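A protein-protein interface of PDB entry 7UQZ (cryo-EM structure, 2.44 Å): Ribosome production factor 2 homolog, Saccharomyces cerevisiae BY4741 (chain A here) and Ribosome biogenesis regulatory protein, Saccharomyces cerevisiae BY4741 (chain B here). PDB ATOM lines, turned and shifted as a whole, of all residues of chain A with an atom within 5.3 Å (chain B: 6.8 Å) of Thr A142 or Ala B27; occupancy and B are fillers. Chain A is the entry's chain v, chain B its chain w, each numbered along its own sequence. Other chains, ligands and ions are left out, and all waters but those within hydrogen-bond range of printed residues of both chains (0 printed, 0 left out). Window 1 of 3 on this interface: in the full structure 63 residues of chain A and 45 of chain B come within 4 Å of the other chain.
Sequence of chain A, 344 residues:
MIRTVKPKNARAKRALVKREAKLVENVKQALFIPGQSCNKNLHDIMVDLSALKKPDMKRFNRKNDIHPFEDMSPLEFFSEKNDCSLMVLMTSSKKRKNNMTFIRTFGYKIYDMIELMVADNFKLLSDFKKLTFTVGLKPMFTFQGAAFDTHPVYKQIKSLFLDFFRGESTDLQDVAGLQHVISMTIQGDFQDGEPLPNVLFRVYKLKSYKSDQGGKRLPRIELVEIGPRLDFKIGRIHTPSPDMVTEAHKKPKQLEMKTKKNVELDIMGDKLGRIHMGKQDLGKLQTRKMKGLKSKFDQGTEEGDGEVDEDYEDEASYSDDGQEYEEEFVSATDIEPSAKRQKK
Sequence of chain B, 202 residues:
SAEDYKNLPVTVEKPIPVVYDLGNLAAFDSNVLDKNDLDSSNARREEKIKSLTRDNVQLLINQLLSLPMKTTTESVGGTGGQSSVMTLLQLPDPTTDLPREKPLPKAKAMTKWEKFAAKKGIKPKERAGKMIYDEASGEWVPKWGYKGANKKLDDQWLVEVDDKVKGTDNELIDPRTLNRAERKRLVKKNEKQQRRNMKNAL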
ATOM      1  N   MET A 140      -2.817  -7.504  -0.085  1.00  0.00           N
ATOM      2  CA  MET A 140      -4.173  -7.087  -0.391  1.00  0.00           C
ATOM      3  C   MET A 140      -5.141  -8.178   0.050  1.00  0.00           C
ATOM      4  O   MET A 140      -4.756  -9.327   0.261  1.00  0.00           O
ATOM      5  CB  MET A 140      -4.324  -6.787  -1.880  1.00  0.00           C
ATOM      6  CG  MET A 140      -3.761  -5.433  -2.276  1.00  0.00           C
ATOM      7  SD  MET A 140      -3.397  -5.297  -4.032  1.00  0.00           S
ATOM      8  CE  MET A 140      -1.933  -6.319  -4.134  1.00  0.00           C
ATOM      9  N   PHE A 141      -6.403  -7.802   0.219  1.00  0.00           N
ATOM     10  CA  PHE A 141      -7.414  -8.726   0.713  1.00  0.00           C
ATOM     11  C   PHE A 141      -8.621  -8.729  -0.208  1.00  0.00           C
ATOM     12  O   PHE A 141      -9.053  -7.676  -0.684  1.00  0.00           O
ATOM     13  CB  PHE A 141      -7.867  -8.361   2.128  1.00  0.00           C
ATOM     14  CG  PHE A 141      -6.828  -8.596   3.179  1.00  0.00           C
ATOM     15  CD1 PHE A 141      -6.745  -9.816   3.826  1.00  0.00           C
ATOM     16  CD2 PHE A 141      -5.941  -7.595   3.528  1.00  0.00           C
ATOM     17  CE1 PHE A 141      -5.792 -10.034   4.798  1.00  0.00           C
ATOM     18  CE2 PHE A 141      -4.987  -7.805   4.498  1.00  0.00           C
ATOM     19  CZ  PHE A 141      -4.914  -9.025   5.134  1.00  0.00           C
ATOM     20  N   THR A 142      -9.160  -9.920  -0.457  1.00  0.00           N
ATOM     21  CA  THR A 142     -10.445 -10.069  -1.126  1.00  0.00           C
ATOM     22  C   THR A 142     -11.292 -11.049  -0.331  1.00  0.00           C
ATOM     23  O   THR A 142     -10.798 -12.100   0.094  1.00  0.00           O
ATOM     24  CB  THR A 142     -10.289 -10.548  -2.576  1.00  0.00           C
ATOM     25  OG1 THR A 142      -9.488 -11.732  -2.610  1.00  0.00           O
ATOM     26  CG2 THR A 142      -9.634  -9.475  -3.433  1.00  0.00           C
ATOM     27  N   PHE A 143     -12.556 -10.695  -0.112  1.00  0.00           N
ATOM     28  CA  PHE A 143     -13.506 -11.532   0.611  1.00  0.00           C
ATOM     29  C   PHE A 143     -14.738 -11.727  -0.261  1.00  0.00           C
ATOM     30  O   PHE A 143     -15.398 -10.752  -0.634  1.00  0.00           O
ATOM     31  CB  PHE A 143     -13.892 -10.904   1.952  1.00  0.00           C
ATOM     32  CG  PHE A 143     -12.791 -10.920   2.972  1.00  0.00           C
ATOM     33  CD1 PHE A 143     -12.647 -11.991   3.838  1.00  0.00           C
ATOM     34  CD2 PHE A 143     -11.904  -9.861   3.073  1.00  0.00           C
ATOM     35  CE1 PHE A 143     -11.637 -12.010   4.780  1.00  0.00           C
ATOM     36  CE2 PHE A 143     -10.892  -9.873   4.014  1.00  0.00           C
ATOM     37  CZ  PHE A 143     -10.758 -10.948   4.868  1.00  0.00           C
ATOM     38  N   GLN A 144     -15.046 -12.982  -0.576  1.00  0.00           N
ATOM     39  CA  GLN A 144     -16.182 -13.331  -1.420  1.00  0.00           C
ATOM     40  C   GLN A 144     -17.256 -13.985  -0.563  1.00  0.00           C
ATOM     41  O   GLN A 144     -17.007 -15.017   0.071  1.00  0.00           O
ATOM     42  CB  GLN A 144     -15.762 -14.262  -2.558  1.00  0.00           C
ATOM     43  CG  GLN A 144     -15.004 -13.581  -3.690  1.00  0.00           C
ATOM     44  CD  GLN A 144     -13.542 -13.342  -3.368  1.00  0.00           C
ATOM     45  OE1 GLN A 144     -13.043 -13.770  -2.327  1.00  0.00           O
ATOM     46  NE2 GLN A 144     -12.845 -12.660  -4.269  1.00  0.00           N
ATOM     47  N   VAL A 181      -2.013 -11.134  -2.721  1.00  0.00           N
ATOM     48  CA  VAL A 181      -3.380 -10.946  -2.260  1.00  0.00           C
ATOM     49  C   VAL A 181      -3.866 -12.232  -1.603  1.00  0.00           C
ATOM     50  O   VAL A 181      -3.643 -13.335  -2.117  1.00  0.00           O
ATOM     51  CB  VAL A 181      -4.315 -10.516  -3.416  1.00  0.00           C
ATOM     52  CG1 VAL A 181      -4.168 -11.447  -4.611  1.00  0.00           C
ATOM     53  CG2 VAL A 181      -5.760 -10.444  -2.948  1.00  0.00           C
ATOM     54  N   ILE A 182      -4.502 -12.082  -0.445  1.00  0.00           N
ATOM     55  CA  ILE A 182      -5.148 -13.170   0.274  1.00  0.00           C
ATOM     56  C   ILE A 182      -6.632 -13.146  -0.064  1.00  0.00           C
ATOM     57  O   ILE A 182      -7.301 -12.119   0.116  1.00  0.00           O
ATOM     58  CB  ILE A 182      -4.927 -13.036   1.791  1.00  0.00           C
ATOM     59  CG1 ILE A 182      -3.455 -13.274   2.140  1.00  0.00           C
ATOM     60  CG2 ILE A 182      -5.838 -13.979   2.553  1.00  0.00           C
ATOM     61  CD1 ILE A 182      -3.120 -12.994   3.590  1.00  0.00           C
ATOM     62  N   SER A 183      -7.146 -14.269  -0.555  1.00  0.00           N
ATOM     63  CA  SER A 183      -8.545 -14.390  -0.936  1.00  0.00           C
ATOM     64  C   SER A 183      -9.244 -15.375  -0.010  1.00  0.00           C
ATOM     65  O   SER A 183      -8.781 -16.507   0.168  1.00  0.00           O
ATOM     66  CB  SER A 183      -8.684 -14.840  -2.391  1.00  0.00           C
ATOM     67  OG  SER A 183      -8.139 -16.129  -2.581  1.00  0.00           O
ATOM     68  N   MET A 184     -10.355 -14.933   0.576  1.00  0.00           N
ATOM     69  CA  MET A 184     -11.183 -15.743   1.462  1.00  0.00           C
ATOM     70  C   MET A 184     -12.580 -15.800   0.860  1.00  0.00           C
ATOM     71  O   MET A 184     -13.299 -14.796   0.856  1.00  0.00           O
ATOM     72  CB  MET A 184     -11.216 -15.153   2.870  1.00  0.00           C
ATOM     73  CG  MET A 184      -9.851 -14.992   3.509  1.00  0.00           C
ATOM     74  SD  MET A 184      -9.296 -16.502   4.307  1.00  0.00           S
ATOM     75  CE  MET A 184     -10.486 -16.624   5.635  1.00  0.00           C
ATOM     76  N   VAL B  18     -18.846  -3.711  -5.802  1.00  0.00           N
ATOM     77  CA  VAL B  18     -17.847  -4.065  -4.801  1.00  0.00           C
ATOM     78  C   VAL B  18     -17.530  -2.850  -3.940  1.00  0.00           C
ATOM     79  O   VAL B  18     -17.346  -1.736  -4.448  1.00  0.00           O
ATOM     80  CB  VAL B  18     -16.580  -4.604  -5.490  1.00  0.00           C
ATOM     81  CG1 VAL B  18     -15.532  -5.023  -4.466  1.00  0.00           C
ATOM     82  CG2 VAL B  18     -16.925  -5.759  -6.411  1.00  0.00           C
ATOM     83  N   VAL B  19     -17.463  -3.055  -2.626  1.00  0.00           N
ATOM     84  CA  VAL B  19     -17.082  -1.998  -1.697  1.00  0.00           C
ATOM     85  C   VAL B  19     -15.601  -2.148  -1.379  1.00  0.00           C
ATOM     86  O   VAL B  19     -15.043  -3.249  -1.420  1.00  0.00           O
ATOM     87  CB  VAL B  19     -17.934  -2.013  -0.410  1.00  0.00           C
ATOM     88  CG1 VAL B  19     -19.358  -1.580  -0.716  1.00  0.00           C
ATOM     89  CG2 VAL B  19     -17.925  -3.389   0.223  1.00  0.00           C
ATOM     90  N   TYR B  20     -14.957  -1.022  -1.073  1.00  0.00           N
ATOM     91  CA  TYR B  20     -13.515  -0.983  -0.884  1.00  0.00           C
ATOM     92  C   TYR B  20     -13.168  -0.380   0.468  1.00  0.00           C
ATOM     93  O   TYR B  20     -13.803   0.581   0.913  1.00  0.00           O
ATOM     94  CB  TYR B  20     -12.827  -0.164  -1.981  1.00  0.00           C
ATOM     95  CG  TYR B  20     -13.208  -0.551  -3.388  1.00  0.00           C
ATOM     96  CD1 TYR B  20     -12.612  -1.635  -4.015  1.00  0.00           C
ATOM     97  CD2 TYR B  20     -14.154   0.179  -4.094  1.00  0.00           C
ATOM     98  CE1 TYR B  20     -12.954  -1.989  -5.303  1.00  0.00           C
ATOM     99  CE2 TYR B  20     -14.503  -0.166  -5.383  1.00  0.00           C
ATOM    100  CZ  TYR B  20     -13.900  -1.250  -5.982  1.00  0.00           C
ATOM    101  OH  TYR B  20     -14.244  -1.596  -7.267  1.00  0.00           O
ATOM    102  N   ASP B  21     -12.157  -0.954   1.114  1.00  0.00           N
ATOM    103  CA  ASP B  21     -11.503  -0.386   2.288  1.00  0.00           C
ATOM    104  C   ASP B  21     -10.039  -0.234   1.885  1.00  0.00           C
ATOM    105  O   ASP B  21      -9.241  -1.163   2.026  1.00  0.00           O
ATOM    106  CB  ASP B  21     -11.673  -1.272   3.519  1.00  0.00           C
ATOM    107  CG  ASP B  21     -11.126  -0.632   4.780  1.00  0.00           C
ATOM    108  OD1 ASP B  21     -10.801   0.573   4.746  1.00  0.00           O
ATOM    109  OD2 ASP B  21     -11.017  -1.335   5.805  1.00  0.00           O
ATOM    110  N   ASN B  24      -6.947  -0.706   4.434  1.00  0.00           N
ATOM    111  CA  ASN B  24      -6.505  -2.078   4.632  1.00  0.00           C
ATOM    112  C   ASN B  24      -6.203  -2.796   3.324  1.00  0.00           C
ATOM    113  O   ASN B  24      -5.843  -3.977   3.359  1.00  0.00           O
ATOM    114  CB  ASN B  24      -7.563  -2.869   5.408  1.00  0.00           C
ATOM    115  CG  ASN B  24      -7.960  -2.199   6.704  1.00  0.00           C
ATOM    116  OD1 ASN B  24      -7.135  -1.587   7.379  1.00  0.00           O
ATOM    117  ND2 ASN B  24      -9.234  -2.311   7.058  1.00  0.00           N
ATOM    118  N   LEU B  25      -6.340  -2.108   2.186  1.00  0.00           N
ATOM    119  CA  LEU B  25      -6.167  -2.696   0.854  1.00  0.00           C
ATOM    120  C   LEU B  25      -7.083  -3.902   0.654  1.00  0.00           C
ATOM    121  O   LEU B  25      -6.670  -4.946   0.145  1.00  0.00           O
ATOM    122  CB  LEU B  25      -4.705  -3.076   0.598  1.00  0.00           C
ATOM    123  CG  LEU B  25      -3.637  -2.012   0.857  1.00  0.00           C
ATOM    124  CD1 LEU B  25      -2.247  -2.583   0.631  1.00  0.00           C
ATOM    125  CD2 LEU B  25      -3.862  -0.798  -0.022  1.00  0.00           C
ATOM    126  N   ALA B  26      -8.345  -3.761   1.056  1.00  0.00           N
ATOM    127  CA  ALA B  26      -9.301  -4.855   1.012  1.00  0.00           C
ATOM    128  C   ALA B  26     -10.497  -4.491   0.142  1.00  0.00           C
ATOM    129  O   ALA B  26     -10.904  -3.329   0.068  1.00  0.00           O
ATOM    130  CB  ALA B  26      -9.776  -5.225   2.423  1.00  0.00           C
ATOM    131  N   ALA B  27     -11.052  -5.499  -0.525  1.00  0.00           N
ATOM    132  CA  ALA B  27     -12.255  -5.345  -1.331  1.00  0.00           C
ATOM    133  C   ALA B  27     -13.256  -6.421  -0.944  1.00  0.00           C
ATOM    134  O   ALA B  27     -12.881  -7.579  -0.734  1.00  0.00           O
ATOM    135  CB  ALA B  27     -11.944  -5.427  -2.830  1.00  0.00           C
ATOM    136  N   PHE B  28     -14.528  -6.039  -0.845  1.00  0.00           N
ATOM    137  CA  PHE B  28     -15.599  -6.950  -0.460  1.00  0.00           C
ATOM    138  C   PHE B  28     -16.684  -6.922  -1.526  1.00  0.00           C
ATOM    139  O   PHE B  28     -17.233  -5.857  -1.833  1.00  0.00           O
ATOM    140  CB  PHE B  28     -16.183  -6.570   0.903  1.00  0.00           C
ATOM    141  CG  PHE B  28     -15.160  -6.092   1.893  1.00  0.00           C
ATOM    142  CD1 PHE B  28     -14.383  -6.996   2.598  1.00  0.00           C
ATOM    143  CD2 PHE B  28     -14.983  -4.738   2.127  1.00  0.00           C
ATOM    144  CE1 PHE B  28     -13.443  -6.557   3.511  1.00  0.00           C
ATOM    145  CE2 PHE B  28     -14.046  -4.293   3.039  1.00  0.00           C
ATOM    146  CZ  PHE B  28     -13.276  -5.204   3.732  1.00  0.00           C
ATOM    147  N   ASP B  29     -17.000  -8.090  -2.080  1.00  0.00           N
ATOM    148  CA  ASP B  29     -18.112  -8.251  -3.006  1.00  0.00           C
ATOM    149  C   ASP B  29     -19.106  -9.239  -2.415  1.00  0.00           C
ATOM    150  O   ASP B  29     -18.720 -10.325  -1.971  1.00  0.00           O
ATOM    151  CB  ASP B  29     -17.636  -8.729  -4.381  1.00  0.00           C
ATOM    152  CG  ASP B  29     -16.687  -9.904  -4.292  1.00  0.00           C
ATOM    153  OD1 ASP B  29     -15.846  -9.920  -3.370  1.00  0.00           O
ATOM    154  OD2 ASP B  29     -16.781 -10.810  -5.147  1.00  0.00           O
ATOM    155  N   LEU B  52     -12.678 -15.020 -10.184  1.00  0.00           N
ATOM    156  CA  LEU B  52     -13.339 -14.065  -9.295  1.00  0.00           C
ATOM    157  C   LEU B  52     -12.323 -13.212  -8.538  1.00  0.00           C
ATOM    158  O   LEU B  52     -12.491 -11.988  -8.412  1.00  0.00           O
ATOM    159  CB  LEU B  52     -14.257 -14.803  -8.320  1.00  0.00           C
ATOM    160  CG  LEU B  52     -15.471 -15.498  -8.939  1.00  0.00           C
ATOM    161  CD1 LEU B  52     -16.298 -16.202  -7.871  1.00  0.00           C
ATOM    162  CD2 LEU B  52     -16.322 -14.503  -9.715  1.00  0.00           C
ATOM    163  N   THR B  53     -11.255 -13.840  -8.036  1.00  0.00           N
ATOM    164  CA  THR B  53     -10.208 -13.098  -7.347  1.00  0.00           C
ATOM    165  C   THR B  53      -9.488 -12.152  -8.298  1.00  0.00           C
ATOM    166  O   THR B  53      -9.099 -11.050  -7.904  1.00  0.00           O
ATOM    167  CB  THR B  53      -9.219 -14.068  -6.699  1.00  0.00           C
ATOM    168  OG1 THR B  53      -9.941 -15.073  -5.977  1.00  0.00           O
ATOM    169  CG2 THR B  53      -8.301 -13.333  -5.735  1.00  0.00           C
ATOM    170  N   ASN B  56     -11.742  -9.102  -8.674  1.00  0.00           N
ATOM    171  CA  ASN B  56     -11.730  -8.269  -7.474  1.00  0.00           C
ATOM    172  C   ASN B  56     -10.404  -7.532  -7.315  1.00  0.00           C
ATOM    173  O   ASN B  56     -10.384  -6.347  -6.957  1.00  0.00           O
ATOM    174  CB  ASN B  56     -12.030  -9.120  -6.242  1.00  0.00           C
ATOM    175  CG  ASN B  56     -13.446  -9.658  -6.240  1.00  0.00           C
ATOM    176  OD1 ASN B  56     -13.681 -10.822  -5.914  1.00  0.00           O
ATOM    177  ND2 ASN B  56     -14.399  -8.813  -6.612  1.00  0.00           N
ATOM    178  N   VAL B  57      -9.287  -8.213  -7.584  1.00  0.00           N
ATOM    179  CA  VAL B  57      -7.978  -7.577  -7.488  1.00  0.00           C
ATOM    180  C   VAL B  57      -7.825  -6.505  -8.560  1.00  0.00           C
ATOM    181  O   VAL B  57      -7.230  -5.452  -8.315  1.00  0.00           O
ATOM    182  CB  VAL B  57      -6.867  -8.641  -7.563  1.00  0.00           C
ATOM    183  CG1 VAL B  57      -5.504  -8.005  -7.777  1.00  0.00           C
ATOM    184  CG2 VAL B  57      -6.849  -9.461  -6.291  1.00  0.00           C
ATOM    185  N   LEU B  59     -10.271  -4.633  -9.783  1.00  0.00           N
ATOM    186  CA  LEU B  59     -11.023  -3.474  -9.305  1.00  0.00           C
ATOM    187  C   LEU B  59     -10.285  -2.752  -8.178  1.00  0.00           C
ATOM    188  O   LEU B  59     -10.251  -1.511  -8.134  1.00  0.00           O
ATOM    189  CB  LEU B  59     -12.416  -3.904  -8.849  1.00  0.00           C
ATOM    190  CG  LEU B  59     -13.376  -4.360  -9.952  1.00  0.00           C
ATOM    191  CD1 LEU B  59     -14.718  -4.767  -9.368  1.00  0.00           C
ATOM    192  CD2 LEU B  59     -13.555  -3.267 -10.993  1.00  0.00           C
ATOM    193  N   LEU B  60      -9.686  -3.513  -7.257  1.00  0.00           N
ATOM    194  CA  LEU B  60      -8.939  -2.907  -6.159  1.00  0.00           C
ATOM    195  C   LEU B  60      -7.732  -2.128  -6.668  1.00  0.00           C
ATOM    196  O   LEU B  60      -7.445  -1.025  -6.187  1.00  0.00           O
ATOM    197  CB  LEU B  60      -8.505  -3.986  -5.169  1.00  0.00           C
ATOM    198  CG  LEU B  60      -7.694  -3.533  -3.958  1.00  0.00           C
ATOM    199  CD1 LEU B  60      -8.492  -2.552  -3.115  1.00  0.00           C
ATOM    200  CD2 LEU B  60      -7.280  -4.735  -3.134  1.00  0.00           C
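Among the printed residues, pairs that only touch across the chains: Met A140 with Leu B25 (3.3 Å), Met A140 with Leu B60 (3.7 Å), Phe A141 with Asn B24 (3.6 Å), Phe A141 with Ala B26 (3.3 Å), Thr A142 with Ala B27 (3.5 Å), Thr A142 with Thr B53 (3.7 Å), Thr A142 with Asn B56 (3.7 Å), Thr A142 with Val B57 (3.99 Å), Phe A143 with Phe B28 (3.7 Å), Gln A144 with Asp B29 (3.6 Å), Val A181 with Val B57 (3.7 Å) and Ser A183 with Thr B53 (3.7 Å).
N of Phe A143 lies within hydrogen-bond range of O of Ala B27 (3.2 Å).
The backbone carbonyl oxygen (O) of Leu B25 is in hydrogen-bond range of the backbone NH (N) of Phe A141 (2.9 Å).
N of Asp B29 is in hydrogen-bond range of O of Phe A143 (3.4 Å).
The backbone carbonyl oxygen (O) of Phe A141 sits at hydrogen-bond distance from the backbone NH (N) of Ala B27 (3.0 Å).
The side-chain amide oxygen (OD1) of Asn B56 lies within hydrogen-bond range of the side-chain amide nitrogen (NE2) of Gln A144.
Printed residues of chain B within 4 Å of Thr A142: Ala B27 (3.5 Å), Thr B53 (3.7 Å), Asn B56 (3.7 Å) and Val B57 (3.99 Å).
Of the printed residues of chain A, Ala B27 touches Phe A141 (3.0 Å), Thr A142 (3.5 Å) and Phe A143 (3.2 Å).
Of the printed residues of chain A, Asp B29 touches Phe A143 (2.9 Å) and Gln A144 (3.6 Å).
Of the printed residues of chain A, Thr B53 touches Thr A142 (3.7 Å) and Ser A183 (3.7 Å).
The nearest printed residue of chain B that does not touch Thr A142 is Ala B26 (5.3 Å).
The nearest printed residue of chain A that does not touch Ala B27 is Gln A144 (5.8 Å).
The nearest printed residue of chain A that does not touch Ala B26 is Phe A143 (5.0 Å).
Of the 9 printed residues of chain A, 7 touch a printed residue of chain B.
Hydrophobic or aromatic side chains of chain A within 4 Å of the printed part of chain B: Met A140, Phe A141, Phe A143 and Val A181.
Of the 16 printed residues of chain B, 10 touch a printed residue of chain A.
Hydrophobic or aromatic side chains of chain B that line the printed part of chain A: Leu B25, Ala B26, Phe B28, Val B57 and Leu B60.
Among the printed residues, 17 pairs touch across the chains.
Among the printed residues, no Asp or Glu carboxylate lies within 4 Å of a Lys or Arg side-chain nitrogen of the other chain.
The backbone carbonyl oxygen (O) of Val B19 sits at hydrogen-bond distance from the backbone NH (N) of Phe B28 (2.9 Å).
N of Asp B21 sits at hydrogen-bond distance from O of Ala B26 (2.9 Å).
The side-chain carboxylate (OD2) of Asp B29 lies close to the side-chain amide oxygen (OD1) of Asn B56 (3.2 Å).
N of Ile A182 sits at hydrogen-bond distance from O of Met A140.
The backbone NH of Met A184 lies within hydrogen-bond range of the backbone carbonyl oxygen of Thr A142, 2.9 Å away.
The backbone NH of Gln A144 is in hydrogen-bond range of the backbone carbonyl oxygen of Met A184 (2.9 Å).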
